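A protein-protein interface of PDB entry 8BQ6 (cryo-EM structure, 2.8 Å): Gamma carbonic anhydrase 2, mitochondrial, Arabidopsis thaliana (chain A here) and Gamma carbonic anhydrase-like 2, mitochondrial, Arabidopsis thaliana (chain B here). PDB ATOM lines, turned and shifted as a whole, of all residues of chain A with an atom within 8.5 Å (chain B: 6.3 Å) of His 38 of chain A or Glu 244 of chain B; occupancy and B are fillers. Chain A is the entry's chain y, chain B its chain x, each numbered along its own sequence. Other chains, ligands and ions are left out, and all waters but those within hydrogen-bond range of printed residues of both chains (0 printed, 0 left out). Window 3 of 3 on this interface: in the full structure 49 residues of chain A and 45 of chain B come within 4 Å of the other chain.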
ATOM      1  N   ARG A  16       6.827  -0.523   2.619  1.00  0.00           N
ATOM      2  CA  ARG A  16       6.164  -0.583   1.319  1.00  0.00           C
ATOM      3  C   ARG A  16       6.249  -1.978   0.720  1.00  0.00           C
ATOM      4  O   ARG A  16       5.260  -2.495   0.184  1.00  0.00           O
ATOM      5  CB  ARG A  16       6.788   0.422   0.360  1.00  0.00           C
ATOM      6  CG  ARG A  16       6.508   1.853   0.697  1.00  0.00           C
ATOM      7  CD  ARG A  16       6.706   2.721  -0.514  1.00  0.00           C
ATOM      8  NE  ARG A  16       5.699   2.457  -1.531  1.00  0.00           N
ATOM      9  CZ  ARG A  16       5.812   2.811  -2.803  1.00  0.00           C
ATOM     10  NH1 ARG A  16       6.897   3.414  -3.259  1.00  0.00           N
ATOM     11  NH2 ARG A  16       4.806   2.568  -3.636  1.00  0.00           N
ATOM     12  N   GLN A  20       2.970  -4.296  -0.218  1.00  0.00           N
ATOM     13  CA  GLN A  20       2.667  -4.836  -1.538  1.00  0.00           C
ATOM     14  C   GLN A  20       2.674  -6.363  -1.540  1.00  0.00           C
ATOM     15  O   GLN A  20       1.867  -6.983  -2.245  1.00  0.00           O
ATOM     16  CB  GLN A  20       3.643  -4.271  -2.570  1.00  0.00           C
ATOM     17  CG  GLN A  20       3.715  -2.751  -2.539  1.00  0.00           C
ATOM     18  CD  GLN A  20       4.289  -2.135  -3.804  1.00  0.00           C
ATOM     19  OE1 GLN A  20       4.879  -2.820  -4.639  1.00  0.00           O
ATOM     20  NE2 GLN A  20       4.123  -0.827  -3.943  1.00  0.00           N
ATOM     21  N   ARG A  34     -10.849 -10.918  -9.083  1.00  0.00           N
ATOM     22  CA  ARG A  34     -11.028  -9.453  -9.251  1.00  0.00           C
ATOM     23  C   ARG A  34     -10.167  -8.928 -10.395  1.00  0.00           C
ATOM     24  O   ARG A  34      -8.953  -9.176 -10.395  1.00  0.00           O
ATOM     25  CB  ARG A  34     -10.706  -8.689  -7.963  1.00  0.00           C
ATOM     26  CG  ARG A  34     -11.550  -7.437  -7.775  1.00  0.00           C
ATOM     27  CD  ARG A  34     -10.868  -6.388  -6.924  1.00  0.00           C
ATOM     28  NE  ARG A  34     -11.644  -5.157  -6.884  1.00  0.00           N
ATOM     29  CZ  ARG A  34     -11.305  -4.026  -7.493  1.00  0.00           C
ATOM     30  NH1 ARG A  34     -10.192  -3.956  -8.205  1.00  0.00           N
ATOM     31  NH2 ARG A  34     -12.088  -2.969  -7.394  1.00  0.00           N
ATOM     32  N   ILE A  35     -10.798  -8.220 -11.330  1.00  0.00           N
ATOM     33  CA  ILE A  35     -10.020  -7.610 -12.397  1.00  0.00           C
ATOM     34  C   ILE A  35      -9.384  -6.330 -11.873  1.00  0.00           C
ATOM     35  O   ILE A  35     -10.059  -5.474 -11.289  1.00  0.00           O
ATOM     36  CB  ILE A  35     -10.909  -7.354 -13.623  1.00  0.00           C
ATOM     37  CG1 ILE A  35     -11.325  -8.684 -14.253  1.00  0.00           C
ATOM     38  CG2 ILE A  35     -10.176  -6.536 -14.653  1.00  0.00           C
ATOM     39  CD1 ILE A  35     -12.443  -8.571 -15.250  1.00  0.00           C
ATOM     40  N   GLU A  36      -8.071  -6.208 -12.057  1.00  0.00           N
ATOM     41  CA  GLU A  36      -7.322  -5.091 -11.500  1.00  0.00           C
ATOM     42  C   GLU A  36      -7.635  -3.794 -12.236  1.00  0.00           C
ATOM     43  O   GLU A  36      -7.719  -3.762 -13.466  1.00  0.00           O
ATOM     44  CB  GLU A  36      -5.819  -5.377 -11.564  1.00  0.00           C
ATOM     45  CG  GLU A  36      -5.290  -6.173 -10.374  1.00  0.00           C
ATOM     46  CD  GLU A  36      -3.815  -6.547 -10.495  1.00  0.00           C
ATOM     47  OE1 GLU A  36      -3.238  -6.423 -11.597  1.00  0.00           O
ATOM     48  OE2 GLU A  36      -3.229  -6.966  -9.475  1.00  0.00           O
ATOM     49  N   GLU A  37      -7.818  -2.722 -11.469  1.00  0.00           N
ATOM     50  CA  GLU A  37      -7.937  -1.400 -12.058  1.00  0.00           C
ATOM     51  C   GLU A  37      -6.605  -0.993 -12.671  1.00  0.00           C
ATOM     52  O   GLU A  37      -5.539  -1.206 -12.091  1.00  0.00           O
ATOM     53  CB  GLU A  37      -8.359  -0.376 -11.007  1.00  0.00           C
ATOM     54  CG  GLU A  37      -9.756  -0.583 -10.469  1.00  0.00           C
ATOM     55  CD  GLU A  37      -9.879  -0.159  -9.025  1.00  0.00           C
ATOM     56  OE1 GLU A  37     -10.749  -0.701  -8.314  1.00  0.00           O
ATOM     57  OE2 GLU A  37      -9.107   0.722  -8.600  1.00  0.00           O
ATOM     58  N   HIS A  38      -6.671  -0.400 -13.856  1.00  0.00           N
ATOM     59  CA  HIS A  38      -5.466  -0.053 -14.587  1.00  0.00           C
ATOM     60  C   HIS A  38      -5.476   1.434 -14.905  1.00  0.00           C
ATOM     61  O   HIS A  38      -6.448   2.146 -14.642  1.00  0.00           O
ATOM     62  CB  HIS A  38      -5.336  -0.890 -15.865  1.00  0.00           C
ATOM     63  CG  HIS A  38      -4.722  -2.238 -15.644  1.00  0.00           C
ATOM     64  ND1 HIS A  38      -4.197  -2.627 -14.430  1.00  0.00           N
ATOM     65  CD2 HIS A  38      -4.538  -3.282 -16.486  1.00  0.00           C
ATOM     66  CE1 HIS A  38      -3.718  -3.853 -14.533  1.00  0.00           C
ATOM     67  NE2 HIS A  38      -3.912  -4.274 -15.770  1.00  0.00           N
ATOM     68  N   LEU A  39      -4.363   1.897 -15.468  1.00  0.00           N
ATOM     69  CA  LEU A  39      -4.273   3.265 -15.955  1.00  0.00           C
ATOM     70  C   LEU A  39      -5.324   3.510 -17.029  1.00  0.00           C
ATOM     71  O   LEU A  39      -5.765   2.582 -17.713  1.00  0.00           O
ATOM     72  CB  LEU A  39      -2.882   3.516 -16.524  1.00  0.00           C
ATOM     73  CG  LEU A  39      -2.312   4.930 -16.545  1.00  0.00           C
ATOM     74  CD1 LEU A  39      -2.256   5.530 -15.161  1.00  0.00           C
ATOM     75  CD2 LEU A  39      -0.940   4.887 -17.178  1.00  0.00           C
ATOM     76  N   SER A  40      -5.719   4.770 -17.183  1.00  0.00           N
ATOM     77  CA  SER A  40      -6.798   5.104 -18.102  1.00  0.00           C
ATOM     78  C   SER A  40      -6.317   5.053 -19.544  1.00  0.00           C
ATOM     79  O   SER A  40      -5.315   5.678 -19.901  1.00  0.00           O
ATOM     80  CB  SER A  40      -7.355   6.488 -17.783  1.00  0.00           C
ATOM     81  OG  SER A  40      -8.667   6.635 -18.295  1.00  0.00           O
ATOM     82  N   ARG A  41      -7.067   4.344 -20.382  1.00  0.00           N
ATOM     83  CA  ARG A  41      -6.692   4.232 -21.815  1.00  0.00           C
ATOM     84  C   ARG A  41      -7.666   5.030 -22.688  1.00  0.00           C
ATOM     85  O   ARG A  41      -7.484   5.023 -23.914  1.00  0.00           O
ATOM     86  CB  ARG A  41      -6.638   2.759 -22.222  1.00  0.00           C
ATOM     87  CG  ARG A  41      -5.445   2.016 -21.637  1.00  0.00           C
ATOM     88  CD  ARG A  41      -4.972   0.859 -22.495  1.00  0.00           C
ATOM     89  NE  ARG A  41      -4.630   1.263 -23.851  1.00  0.00           N
ATOM     90  CZ  ARG A  41      -3.409   1.218 -24.371  1.00  0.00           C
ATOM     91  NH1 ARG A  41      -2.393   0.788 -23.643  1.00  0.00           N
ATOM     92  NH2 ARG A  41      -3.205   1.609 -25.614  1.00  0.00           N
ATOM     93  N   THR B 240      -5.289   1.259  -6.495  1.00  0.00           N
ATOM     94  CA  THR B 240      -3.872   0.977  -6.672  1.00  0.00           C
ATOM     95  C   THR B 240      -3.338   1.516  -7.994  1.00  0.00           C
ATOM     96  O   THR B 240      -2.264   1.095  -8.438  1.00  0.00           O
ATOM     97  CB  THR B 240      -3.608  -0.526  -6.552  1.00  0.00           C
ATOM     98  OG1 THR B 240      -4.654  -1.258  -7.201  1.00  0.00           O
ATOM     99  CG2 THR B 240      -3.538  -0.941  -5.095  1.00  0.00           C
ATOM    100  N   ILE B 241      -4.058   2.453  -8.616  1.00  0.00           N
ATOM    101  CA  ILE B 241      -3.607   3.043  -9.876  1.00  0.00           C
ATOM    102  C   ILE B 241      -2.313   3.814  -9.674  1.00  0.00           C
ATOM    103  O   ILE B 241      -1.453   3.858 -10.564  1.00  0.00           O
ATOM    104  CB  ILE B 241      -4.700   3.952 -10.468  1.00  0.00           C
ATOM    105  CG1 ILE B 241      -6.003   3.192 -10.633  1.00  0.00           C
ATOM    106  CG2 ILE B 241      -4.278   4.466 -11.826  1.00  0.00           C
ATOM    107  CD1 ILE B 241      -5.873   2.073 -11.562  1.00  0.00           C
ATOM    108  N   TYR B 242      -2.161   4.453  -8.511  1.00  0.00           N
ATOM    109  CA  TYR B 242      -0.998   5.305  -8.293  1.00  0.00           C
ATOM    110  C   TYR B 242       0.303   4.525  -8.437  1.00  0.00           C
ATOM    111  O   TYR B 242       1.326   5.099  -8.815  1.00  0.00           O
ATOM    112  CB  TYR B 242      -1.090   5.990  -6.929  1.00  0.00           C
ATOM    113  CG  TYR B 242      -0.944   5.084  -5.732  1.00  0.00           C
ATOM    114  CD1 TYR B 242      -2.034   4.396  -5.224  1.00  0.00           C
ATOM    115  CD2 TYR B 242       0.272   4.945  -5.089  1.00  0.00           C
ATOM    116  CE1 TYR B 242      -1.909   3.580  -4.126  1.00  0.00           C
ATOM    117  CE2 TYR B 242       0.408   4.134  -3.987  1.00  0.00           C
ATOM    118  CZ  TYR B 242      -0.686   3.451  -3.509  1.00  0.00           C
ATOM    119  OH  TYR B 242      -0.562   2.634  -2.410  1.00  0.00           O
ATOM    120  N   LEU B 243       0.273   3.216  -8.191  1.00  0.00           N
ATOM    121  CA  LEU B 243       1.448   2.385  -8.442  1.00  0.00           C
ATOM    122  C   LEU B 243       1.750   2.275  -9.934  1.00  0.00           C
ATOM    123  O   LEU B 243       2.919   2.319 -10.349  1.00  0.00           O
ATOM    124  CB  LEU B 243       1.234   1.007  -7.825  1.00  0.00           C
ATOM    125  CG  LEU B 243       1.241   1.022  -6.298  1.00  0.00           C
ATOM    126  CD1 LEU B 243       1.365  -0.377  -5.763  1.00  0.00           C
ATOM    127  CD2 LEU B 243       2.379   1.885  -5.791  1.00  0.00           C
ATOM    128  N   GLU B 244       0.710   2.121 -10.760  1.00  0.00           N
ATOM    129  CA  GLU B 244       0.910   2.115 -12.205  1.00  0.00           C
ATOM    130  C   GLU B 244       1.461   3.450 -12.680  1.00  0.00           C
ATOM    131  O   GLU B 244       2.344   3.498 -13.545  1.00  0.00           O
ATOM    132  CB  GLU B 244      -0.402   1.813 -12.925  1.00  0.00           C
ATOM    133  CG  GLU B 244      -1.137   0.570 -12.472  1.00  0.00           C
ATOM    134  CD  GLU B 244      -0.918  -0.606 -13.393  1.00  0.00           C
ATOM    135  OE1 GLU B 244       0.104  -1.297 -13.256  1.00  0.00           O
ATOM    136  OE2 GLU B 244      -1.761  -0.823 -14.284  1.00  0.00           O
ATOM    137  N   VAL B 245       0.940   4.547 -12.130  1.00  0.00           N
ATOM    138  CA  VAL B 245       1.463   5.869 -12.468  1.00  0.00           C
ATOM    139  C   VAL B 245       2.926   5.979 -12.066  1.00  0.00           C
ATOM    140  O   VAL B 245       3.745   6.549 -12.796  1.00  0.00           O
ATOM    141  CB  VAL B 245       0.611   6.966 -11.806  1.00  0.00           C
ATOM    142  CG1 VAL B 245       0.963   8.323 -12.377  1.00  0.00           C
ATOM    143  CG2 VAL B 245      -0.860   6.678 -11.997  1.00  0.00           C
ATOM    144  N   GLU B 246       3.275   5.443 -10.895  1.00  0.00           N
ATOM    145  CA  GLU B 246       4.649   5.506 -10.413  1.00  0.00           C
ATOM    146  C   GLU B 246       5.601   4.759 -11.337  1.00  0.00           C
ATOM    147  O   GLU B 246       6.698   5.243 -11.642  1.00  0.00           O
ATOM    148  CB  GLU B 246       4.722   4.932  -9.002  1.00  0.00           C
ATOM    149  CG  GLU B 246       5.837   5.482  -8.155  1.00  0.00           C
ATOM    150  CD  GLU B 246       5.931   4.764  -6.829  1.00  0.00           C
ATOM    151  OE1 GLU B 246       5.005   3.988  -6.512  1.00  0.00           O
ATOM    152  OE2 GLU B 246       6.928   4.968  -6.108  1.00  0.00           O
ATOM    153  N   LYS B 247       5.210   3.567 -11.791  1.00  0.00           N
ATOM    154  CA  LYS B 247       6.125   2.843 -12.669  1.00  0.00           C
ATOM    155  C   LYS B 247       6.148   3.441 -14.071  1.00  0.00           C
ATOM    156  O   LYS B 247       7.184   3.391 -14.737  1.00  0.00           O
ATOM    157  CB  LYS B 247       5.785   1.357 -12.733  1.00  0.00           C
ATOM    158  CG  LYS B 247       4.343   1.052 -12.960  1.00  0.00           C
ATOM    159  CD  LYS B 247       4.191  -0.341 -13.524  1.00  0.00           C
ATOM    160  CE  LYS B 247       2.781  -0.574 -13.991  1.00  0.00           C
ATOM    161  NZ  LYS B 247       2.620  -1.873 -14.707  1.00  0.00           N
ATOM    162  N   PHE B 248       5.032   4.015 -14.532  1.00  0.00           N
ATOM    163  CA  PHE B 248       5.039   4.763 -15.787  1.00  0.00           C
ATOM    164  C   PHE B 248       5.994   5.948 -15.709  1.00  0.00           C
ATOM    165  O   PHE B 248       6.713   6.244 -16.668  1.00  0.00           O
ATOM    166  CB  PHE B 248       3.617   5.232 -16.106  1.00  0.00           C
ATOM    167  CG  PHE B 248       3.387   5.589 -17.550  1.00  0.00           C
ATOM    168  CD1 PHE B 248       3.718   6.840 -18.030  1.00  0.00           C
ATOM    169  CD2 PHE B 248       2.803   4.683 -18.415  1.00  0.00           C
ATOM    170  CE1 PHE B 248       3.494   7.173 -19.353  1.00  0.00           C
ATOM    171  CE2 PHE B 248       2.575   5.013 -19.738  1.00  0.00           C
ATOM    172  CZ  PHE B 248       2.919   6.257 -20.206  1.00  0.00           C
ATOM    173  N   LYS B 249       6.005   6.643 -14.572  1.00  0.00           N
ATOM    174  CA  LYS B 249       6.920   7.763 -14.385  1.00  0.00           C
ATOM    175  C   LYS B 249       8.366   7.289 -14.329  1.00  0.00           C
ATOM    176  O   LYS B 249       9.263   7.928 -14.889  1.00  0.00           O
ATOM    177  CB  LYS B 249       6.557   8.519 -13.111  1.00  0.00           C
ATOM    178  CG  LYS B 249       5.681   9.722 -13.338  1.00  0.00           C
ATOM    179  CD  LYS B 249       5.239  10.310 -12.022  1.00  0.00           C
ATOM    180  CE  LYS B 249       6.183  11.413 -11.584  1.00  0.00           C
ATOM    181  NZ  LYS B 249       7.310  10.882 -10.768  1.00  0.00           N
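Of chain B, only Ile 241 (3.1 Å) and Glu 244 (3.0 Å) come within 4 Å of His 38 of chain A. Glu 244 of chain B touches just these residues of chain A: His 38 (3.0 Å) and Leu 39 (3.9 Å). Of the printed residues of chain A, Leu 243 of chain B touches Arg 16 (3.3 Å) and Gln 20 (3.3 Å). Of the printed residues of chain B, Gln 20 of chain A touches Leu 243 (3.3 Å). Printed residues of chain A within 4 Å of Ile 241 of chain B: Glu 37 and His 38. Lys 247 of chain B touches none of the printed residues of chain A. Ser 40 of chain A touches none of the printed residues of chain B. The nearest printed residue of chain B that does not touch His 38 of chain A is Lys 247 of chain B (6.6 Å).
The guanidinium group of Arg 16 of chain A lies close to the side-chain amide nitrogen of Gln 20 of chain A (3.5 Å). The side-chain carboxylate (OE1) of Glu 37 of chain A is in salt-bridge range of the guanidinium group (NH2) of Arg 34 of chain A (2.8 Å). The side-chain carboxylate (OE1) of Glu 244 of chain B is in salt-bridge range of the side-chain amino group (NZ) of Lys 247 of chain B, 3.0 Å away.
Among the printed residues, pairs that only touch across the chains: Arg 16 of chain A with Leu 243 of chain B, Gln 20 of chain A with Leu 243 of chain B, Glu 37 of chain A with Ile 241 of chain B, His 38 of chain A with Ile 241 of chain B, Leu 39 of chain A with Glu 244 of chain B, Leu 39 of chain A with Val 245 of chain B and Leu 39 of chain A with Phe 248 of chain B.
ND1 of His 38 of chain A is in hydrogen-bond range of OE2 of Glu 244 of chain B (3.0 Å). The side-chain carboxylate (OE1) of Glu 246 of chain B is in salt-bridge range of the guanidinium group (NH2) of Arg 16 of chain A, at 3.2 Å.
Of the 10 printed residues of chain B, 6 touch a printed residue of chain A. Hydrophobic or aromatic side chains of chain B within 4 Å of the printed part of chain A: Ile 241, Leu 243, Val 245 and Phe 248. Along chain B the printed residues that touch a printed residue of chain A span positions 241 to 248. Printed residues of chain A that touch a printed residue of chain B: Arg 16, Gln 20, Glu 37, His 38 and Leu 39. Hydrophobic or aromatic side chains of chain A that line the printed part of chain B: His 38 and Leu 39.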
